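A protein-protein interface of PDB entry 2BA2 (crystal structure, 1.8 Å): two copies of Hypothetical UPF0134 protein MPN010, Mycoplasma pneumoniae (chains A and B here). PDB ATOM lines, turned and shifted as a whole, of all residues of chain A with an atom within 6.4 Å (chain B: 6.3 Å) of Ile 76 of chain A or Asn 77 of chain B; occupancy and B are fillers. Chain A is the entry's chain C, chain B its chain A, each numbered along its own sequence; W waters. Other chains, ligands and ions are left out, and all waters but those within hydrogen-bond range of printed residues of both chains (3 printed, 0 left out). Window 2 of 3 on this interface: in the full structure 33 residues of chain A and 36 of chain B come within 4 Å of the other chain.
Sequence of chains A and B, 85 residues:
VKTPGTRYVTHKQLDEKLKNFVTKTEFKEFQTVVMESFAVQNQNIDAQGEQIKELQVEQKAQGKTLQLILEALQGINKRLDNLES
Of the 11 printed residues of chain B, 5 touch a printed residue of chain A. Hydrophobic or aromatic side chains of chain B that line the printed part of chain A: Leu 73, Ile 76 and Leu 80. Printed residues of chain A that touch a printed residue of chain B: Ala 72, Leu 73, Ile 76, Arg 79 and Leu 80. Among the printed residues, 10 pairs touch across the chains. Among the printed residues, Asp or Glu carboxylates within 4 Å of a Lys or Arg side-chain nitrogen of the other chain: Arg 79 of chain A with Asp 81 of chain B (3.1 Å).
CD1 of Leu 73 of chain B touches CB of Ala 72 of chain A (3.9 Å). Leu 73 of chain B touches Leu 73 of chain A. Leu 73 of chain B touches Ile 76 of chain A. Ile 76 of chain A touches Ile 76 of chain B. Ile 76 of chain A touches Asn 77 of chain B (CG1 to ND2, 3.5 Å). Leu 80 of chain B touches Ile 76 of chain A. O of Asn 77 of chain B touches NH2 of Arg 79 of chain A, 3.9 Å away. Arg 79 of chain A touches Leu 80 of chain B (NH2 to CB, 3.4 Å). Leu 80 of chain A touches Leu 80 of chain B (CD2 to CD2, 3.8 Å).
Water W3 bridges the guanidinium group of Arg 79 of chain A and the side-chain amide nitrogen of Asn 77 of chain B. Water W1 bridges the side-chain carboxylate of Asp 81 of chain B (2.7 Å) and the guanidinium group of Arg 79 of chain A (3.2 Å). Water W2 lies within hydrogen-bond range of the side-chain carboxylate of Asp 81 of chain B (2.8 Å), the guanidinium group of Arg 79 of chain A (3.1 Å) and the backbone carbonyl oxygen of Asn 77 of chain B (3.4 Å).
Ile 76 of chain A touches just these residues of chain B: Leu 73 (3.5 Å), Ile 76 (3.7 Å), Asn 77 (3.5 Å) and Leu 80 (3.9 Å). Of chain A, only Ile 76 (3.5 Å) and Arg 79 (3.9 Å) come within 4 Å of Asn 77 of chain B. Printed residues of chain B within 4 Å of Arg 79 of chain A: Asn 77, Leu 80 and Asp 81. Printed residues of chain A within 4 Å of Ile 76 of chain B: Ile 76. Of the printed residues of chain B, Ala 72 of chain A touches Leu 73 (3.9 Å). Of the printed residues of chain A, Leu 73 of chain B touches Ala 72, Leu 73 and Ile 76. Gln 74 of chain A touches none of the printed residues of chain B. Asp 81 of chain A touches none of the printed residues of chain B. The nearest printed residue of chain B that does not touch Ile 76 of chain A is Ala 72 of chain B (6.4 Å). The nearest residue of chain A that does not touch Asn 77 of chain B is Ala 72 of chain A (5.7 Å).
Ile 76 of chain A touches Leu 73 of chain B, but with the chains exchanged Leu 73 of chain A does not touch Ile 76 of chain B (5.8 Å). Ile 76 of chain A touches Leu 80 of chain B, but with the chains exchanged Leu 80 of chain A does not touch Ile 76 of chain B (6.1 Å). Arg 79 of chain A touches Leu 80 of chain B, but with the chains exchanged Leu 80 of chain A does not touch Arg 79 of chain B (7.6 Å). Leu 80 of chain A touches its own counterpart, Leu 80 of chain B. Of the 10 pairs that touch across the chains among the printed residues, 3 have their exchanged pair printed and touching as well.
The side-chain amide nitrogen (ND2) of Asn 77 of chain B sits close to the backbone carbonyl oxygen (O) of Leu 73 of chain B, 3.1 Å away. O of Asn 77 of chain B lies close to OD2 of Asp 81 of chain B (2.6 Å). The side-chain amide nitrogen (ND2) of Asn 77 of chain A lies within hydrogen-bond range of the backbone carbonyl oxygen (O) of Leu 73 of chain A, 3.0 Å away.
OD1 of Asp 81 of chain B lies within salt-bridge range of NH2 of Arg 79 of chain A, 3.1 Å away.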
ATOM      1  N   GLU A  71      -6.069   7.082   4.242  1.00  0.00           N
ATOM      2  CA  GLU A  71      -6.059   6.537   5.592  1.00  0.00           C
ATOM      3  C   GLU A  71      -4.979   7.250   6.410  1.00  0.00           C
ATOM      4  O   GLU A  71      -5.224   7.668   7.540  1.00  0.00           O
ATOM      5  CB  GLU A  71      -5.789   5.027   5.562  1.00  0.00           C
ATOM      6  CG  GLU A  71      -6.725   4.251   4.640  1.00  0.00           C
ATOM      7  CD  GLU A  71      -6.601   2.743   4.789  1.00  0.00           C
ATOM      8  OE1 GLU A  71      -5.462   2.231   4.821  1.00  0.00           O
ATOM      9  OE2 GLU A  71      -7.649   2.066   4.862  1.00  0.00           O
ATOM     10  N   ALA A  72      -3.790   7.391   5.831  1.00  0.00           N
ATOM     11  CA  ALA A  72      -2.682   8.059   6.506  1.00  0.00           C
ATOM     12  C   ALA A  72      -3.086   9.468   6.933  1.00  0.00           C
ATOM     13  O   ALA A  72      -2.771   9.900   8.041  1.00  0.00           O
ATOM     14  CB  ALA A  72      -1.457   8.116   5.588  1.00  0.00           C
ATOM     15  N   LEU A  73      -3.784  10.179   6.054  1.00  0.00           N
ATOM     16  CA  LEU A  73      -4.235  11.534   6.358  1.00  0.00           C
ATOM     17  C   LEU A  73      -5.178  11.540   7.550  1.00  0.00           C
ATOM     18  O   LEU A  73      -5.208  12.491   8.328  1.00  0.00           O
ATOM     19  CB  LEU A  73      -4.949  12.147   5.157  1.00  0.00           C
ATOM     20  CG  LEU A  73      -4.085  12.498   3.947  1.00  0.00           C
ATOM     21  CD1 LEU A  73      -4.968  13.072   2.855  1.00  0.00           C
ATOM     22  CD2 LEU A  73      -3.017  13.500   4.355  1.00  0.00           C
ATOM     23  N   GLN A  74      -5.967  10.482   7.684  1.00  0.00           N
ATOM     24  CA  GLN A  74      -6.894  10.385   8.802  1.00  0.00           C
ATOM     25  C   GLN A  74      -6.091  10.190  10.081  1.00  0.00           C
ATOM     26  O   GLN A  74      -6.423  10.750  11.127  1.00  0.00           O
ATOM     27  CB  GLN A  74      -7.852   9.209   8.602  1.00  0.00           C
ATOM     28  CG  GLN A  74      -8.868   9.039   9.723  1.00  0.00           C
ATOM     29  CD  GLN A  74      -9.726  10.275   9.928  1.00  0.00           C
ATOM     30  OE1 GLN A  74     -10.448  10.700   9.025  1.00  0.00           O
ATOM     31  NE2 GLN A  74      -9.649  10.859  11.119  1.00  0.00           N
ATOM     32  N   GLY A  75      -5.028   9.398   9.990  1.00  0.00           N
ATOM     33  CA  GLY A  75      -4.187   9.149  11.148  1.00  0.00           C
ATOM     34  C   GLY A  75      -3.423  10.395  11.552  1.00  0.00           C
ATOM     35  O   GLY A  75      -3.263  10.683  12.738  1.00  0.00           O
ATOM     36  N   ILE A  76      -2.947  11.140  10.560  1.00  0.00           N
ATOM     37  CA  ILE A  76      -2.211  12.362  10.823  1.00  0.00           C
ATOM     38  C   ILE A  76      -3.127  13.384  11.488  1.00  0.00           C
ATOM     39  O   ILE A  76      -2.711  14.084  12.408  1.00  0.00           O
ATOM     40  CB  ILE A  76      -1.647  12.960   9.517  1.00  0.00           C
ATOM     41  CG1 ILE A  76      -0.520  12.067   8.988  1.00  0.00           C
ATOM     42  CG2 ILE A  76      -1.143  14.379   9.765  1.00  0.00           C
ATOM     43  CD1 ILE A  76      -0.090  12.381   7.565  1.00  0.00           C
ATOM     44  N   ASN A  77      -4.373  13.460  11.026  1.00  0.00           N
ATOM     45  CA  ASN A  77      -5.328  14.406  11.592  1.00  0.00           C
ATOM     46  C   ASN A  77      -5.681  14.053  13.027  1.00  0.00           C
ATOM     47  O   ASN A  77      -5.928  14.938  13.844  1.00  0.00           O
ATOM     48  CB  ASN A  77      -6.600  14.480  10.743  1.00  0.00           C
ATOM     49  CG  ASN A  77      -6.404  15.290   9.473  1.00  0.00           C
ATOM     50  OD1 ASN A  77      -5.682  16.290   9.470  1.00  0.00           O
ATOM     51  ND2 ASN A  77      -7.056  14.874   8.391  1.00  0.00           N
ATOM     52  N   LYS A  78      -5.711  12.762  13.335  1.00  0.00           N
ATOM     53  CA  LYS A  78      -6.012  12.326  14.694  1.00  0.00           C
ATOM     54  C   LYS A  78      -4.861  12.729  15.610  1.00  0.00           C
ATOM     55  O   LYS A  78      -5.077  13.214  16.718  1.00  0.00           O
ATOM     56  CB  LYS A  78      -6.198  10.808  14.749  1.00  0.00           C
ATOM     57  CG  LYS A  78      -7.342  10.292  13.892  1.00  0.00           C
ATOM     58  CD  LYS A  78      -7.586   8.805  14.124  1.00  0.00           C
ATOM     59  CE  LYS A  78      -8.659   8.271  13.185  1.00  0.00           C
ATOM     60  NZ  LYS A  78      -9.922   9.063  13.256  1.00  0.00           N
ATOM     61  N   ARG A  79      -3.631  12.538  15.139  1.00  0.00           N
ATOM     62  CA  ARG A  79      -2.460  12.884  15.935  1.00  0.00           C
ATOM     63  C   ARG A  79      -2.382  14.391  16.149  1.00  0.00           C
ATOM     64  O   ARG A  79      -2.013  14.856  17.227  1.00  0.00           O
ATOM     65  CB  ARG A  79      -1.192  12.358  15.260  1.00  0.00           C
ATOM     66  CG  ARG A  79      -1.142  10.835  15.217  1.00  0.00           C
ATOM     67  CD  ARG A  79       0.014  10.307  14.383  1.00  0.00           C
ATOM     68  NE  ARG A  79       1.319  10.563  14.984  1.00  0.00           N
ATOM     69  CZ  ARG A  79       2.471  10.186  14.438  1.00  0.00           C
ATOM     70  NH1 ARG A  79       2.473   9.542  13.279  1.00  0.00           N
ATOM     71  NH2 ARG A  79       3.618  10.437  15.055  1.00  0.00           N
ATOM     72  N   LEU A  80      -2.745  15.156  15.125  1.00  0.00           N
ATOM     73  CA  LEU A  80      -2.735  16.605  15.239  1.00  0.00           C
ATOM     74  C   LEU A  80      -3.770  17.053  16.260  1.00  0.00           C
ATOM     75  O   LEU A  80      -3.477  17.886  17.114  1.00  0.00           O
ATOM     76  CB  LEU A  80      -3.020  17.258  13.884  1.00  0.00           C
ATOM     77  CG  LEU A  80      -1.828  17.267  12.918  1.00  0.00           C
ATOM     78  CD1 LEU A  80      -2.248  17.866  11.582  1.00  0.00           C
ATOM     79  CD2 LEU A  80      -0.675  18.053  13.531  1.00  0.00           C
ATOM     80  N   ASP A  81      -4.975  16.492  16.171  1.00  0.00           N
ATOM     81  CA  ASP A  81      -6.048  16.836  17.102  1.00  0.00           C
ATOM     82  C   ASP A  81      -5.698  16.420  18.529  1.00  0.00           C
ATOM     83  O   ASP A  81      -6.152  17.040  19.493  1.00  0.00           O
ATOM     84  CB  ASP A  81      -7.362  16.163  16.696  1.00  0.00           C
ATOM     85  CG  ASP A  81      -7.851  16.606  15.329  1.00  0.00           C
ATOM     86  OD1 ASP A  81      -7.808  17.821  15.042  1.00  0.00           O
ATOM     87  OD2 ASP A  81      -8.289  15.738  14.545  1.00  0.00           O
ATOM     88  N   ALA B  72       5.735  13.657   1.104  1.00  0.00           N
ATOM     89  CA  ALA B  72       5.221  14.652   2.034  1.00  0.00           C
ATOM     90  C   ALA B  72       4.773  13.993   3.331  1.00  0.00           C
ATOM     91  O   ALA B  72       5.125  14.448   4.417  1.00  0.00           O
ATOM     92  CB  ALA B  72       4.057  15.403   1.405  1.00  0.00           C
ATOM     93  N   LEU B  73       3.988  12.924   3.205  1.00  0.00           N
ATOM     94  CA  LEU B  73       3.475  12.191   4.355  1.00  0.00           C
ATOM     95  C   LEU B  73       4.571  11.708   5.301  1.00  0.00           C
ATOM     96  O   LEU B  73       4.380  11.689   6.517  1.00  0.00           O
ATOM     97  CB  LEU B  73       2.645  10.991   3.893  1.00  0.00           C
ATOM     98  CG  LEU B  73       1.307  11.279   3.209  1.00  0.00           C
ATOM     99  CD1 LEU B  73       0.622   9.965   2.890  1.00  0.00           C
ATOM    100  CD2 LEU B  73       0.421  12.126   4.113  1.00  0.00           C
ATOM    101  N   GLN B  74       5.714  11.312   4.751  1.00  0.00           N
ATOM    102  CA  GLN B  74       6.806  10.841   5.596  1.00  0.00           C
ATOM    103  C   GLN B  74       7.409  11.999   6.384  1.00  0.00           C
ATOM    104  O   GLN B  74       7.743  11.851   7.560  1.00  0.00           O
ATOM    105  CB  GLN B  74       7.890  10.161   4.755  1.00  0.00           C
ATOM    106  CG  GLN B  74       9.011   9.570   5.595  1.00  0.00           C
ATOM    107  CD  GLN B  74       8.493   8.653   6.693  1.00  0.00           C
ATOM    108  OE1 GLN B  74       7.908   7.605   6.419  1.00  0.00           O
ATOM    109  NE2 GLN B  74       8.703   9.050   7.945  1.00  0.00           N
ATOM    110  N   GLY B  75       7.538  13.153   5.736  1.00  0.00           N
ATOM    111  CA  GLY B  75       8.084  14.316   6.408  1.00  0.00           C
ATOM    112  C   GLY B  75       7.155  14.761   7.521  1.00  0.00           C
ATOM    113  O   GLY B  75       7.603  15.227   8.569  1.00  0.00           O
ATOM    114  N   ILE B  76       5.854  14.617   7.293  1.00  0.00           N
ATOM    115  CA  ILE B  76       4.858  14.994   8.285  1.00  0.00           C
ATOM    116  C   ILE B  76       4.952  14.052   9.488  1.00  0.00           C
ATOM    117  O   ILE B  76       5.040  14.495  10.635  1.00  0.00           O
ATOM    118  CB  ILE B  76       3.430  14.929   7.686  1.00  0.00           C
ATOM    119  CG1 ILE B  76       3.245  16.059   6.667  1.00  0.00           C
ATOM    120  CG2 ILE B  76       2.388  15.042   8.790  1.00  0.00           C
ATOM    121  CD1 ILE B  76       1.931  15.998   5.885  1.00  0.00           C
ATOM    122  N   ASN B  77       4.946  12.753   9.213  1.00  0.00           N
ATOM    123  CA  ASN B  77       5.027  11.740  10.258  1.00  0.00           C
ATOM    124  C   ASN B  77       6.247  11.934  11.140  1.00  0.00           C
ATOM    125  O   ASN B  77       6.200  11.669  12.340  1.00  0.00           O
ATOM    126  CB  ASN B  77       5.060  10.342   9.641  1.00  0.00           C
ATOM    127  CG  ASN B  77       3.744   9.962   9.004  1.00  0.00           C
ATOM    128  OD1 ASN B  77       3.596   8.874   8.449  1.00  0.00           O
ATOM    129  ND2 ASN B  77       2.773  10.859   9.086  1.00  0.00           N
ATOM    130  N   LYS B  78       7.342  12.390  10.541  1.00  0.00           N
ATOM    131  CA  LYS B  78       8.561  12.625  11.301  1.00  0.00           C
ATOM    132  C   LYS B  78       8.398  13.852  12.188  1.00  0.00           C
ATOM    133  O   LYS B  78       8.881  13.869  13.319  1.00  0.00           O
ATOM    134  CB  LYS B  78       9.759  12.810  10.367  1.00  0.00           C
ATOM    135  CG  LYS B  78      10.205  11.532   9.673  1.00  0.00           C
ATOM    136  CD  LYS B  78      11.528  11.735   8.950  1.00  0.00           C
ATOM    137  CE  LYS B  78      12.034  10.439   8.333  1.00  0.00           C
ATOM    138  NZ  LYS B  78      13.342  10.625   7.641  1.00  0.00           N
ATOM    139  N   ARG B  79       7.719  14.876  11.678  1.00  0.00           N
ATOM    140  CA  ARG B  79       7.500  16.093  12.452  1.00  0.00           C
ATOM    141  C   ARG B  79       6.574  15.790  13.624  1.00  0.00           C
ATOM    142  O   ARG B  79       6.644  16.442  14.668  1.00  0.00           O
ATOM    143  CB  ARG B  79       6.903  17.196  11.568  1.00  0.00           C
ATOM    144  CG  ARG B  79       7.882  17.747  10.533  1.00  0.00           C
ATOM    145  CD  ARG B  79       7.212  18.678   9.524  1.00  0.00           C
ATOM    146  NE  ARG B  79       6.796  19.951  10.109  1.00  0.00           N
ATOM    147  CZ  ARG B  79       6.167  20.912   9.436  1.00  0.00           C
ATOM    148  NH1 ARG B  79       5.876  20.745   8.152  1.00  0.00           N
ATOM    149  NH2 ARG B  79       5.831  22.042  10.044  1.00  0.00           N
ATOM    150  N   LEU B  80       5.716  14.788  13.446  1.00  0.00           N
ATOM    151  CA  LEU B  80       4.783  14.373  14.484  1.00  0.00           C
ATOM    152  C   LEU B  80       5.509  13.523  15.527  1.00  0.00           C
ATOM    153  O   LEU B  80       5.229  13.616  16.724  1.00  0.00           O
ATOM    154  CB  LEU B  80       3.630  13.580  13.862  1.00  0.00           C
ATOM    155  CG  LEU B  80       2.604  14.418  13.092  1.00  0.00           C
ATOM    156  CD1 LEU B  80       1.688  13.517  12.280  1.00  0.00           C
ATOM    157  CD2 LEU B  80       1.805  15.255  14.078  1.00  0.00           C
ATOM    158  N   ASP B  81       6.447  12.697  15.067  1.00  0.00           N
ATOM    159  CA  ASP B  81       7.219  11.849  15.969  1.00  0.00           C
ATOM    160  C   ASP B  81       8.033  12.740  16.895  1.00  0.00           C
ATOM    161  O   ASP B  81       8.135  12.479  18.094  1.00  0.00           O
ATOM    162  CB  ASP B  81       8.173  10.939  15.189  1.00  0.00           C
ATOM    163  CG  ASP B  81       7.449   9.971  14.281  1.00  0.00           C
ATOM    164  OD1 ASP B  81       6.484   9.327  14.741  1.00  0.00           O
ATOM    165  OD2 ASP B  81       7.857   9.843  13.109  1.00  0.00           O
ATOM    166  N   ASN B  82       8.614  13.792  16.325  1.00  0.00           N
ATOM    167  CA  ASN B  82       9.414  14.742  17.087  1.00  0.00           C
ATOM    168  C   ASN B  82       8.545  15.459  18.119  1.00  0.00           C
ATOM    169  O   ASN B  82       8.975  15.694  19.248  1.00  0.00           O
ATOM    170  CB  ASN B  82      10.054  15.768  16.150  1.00  0.00           C
ATOM    171  CG  ASN B  82      10.836  16.835  16.896  1.00  0.00           C
ATOM    172  OD1 ASN B  82      10.275  17.596  17.687  1.00  0.00           O
ATOM    173  ND2 ASN B  82      12.140  16.894  16.649  1.00  0.00           N
HETATM  174  O   HOH W   1       5.103   7.980  16.568  1.00  0.00           O
HETATM  175  O   HOH W   2       5.226   8.380  12.391  1.00  0.00           O
HETATM  176  O   HOH W   3       0.911   9.570  11.149  1.00  0.00           O
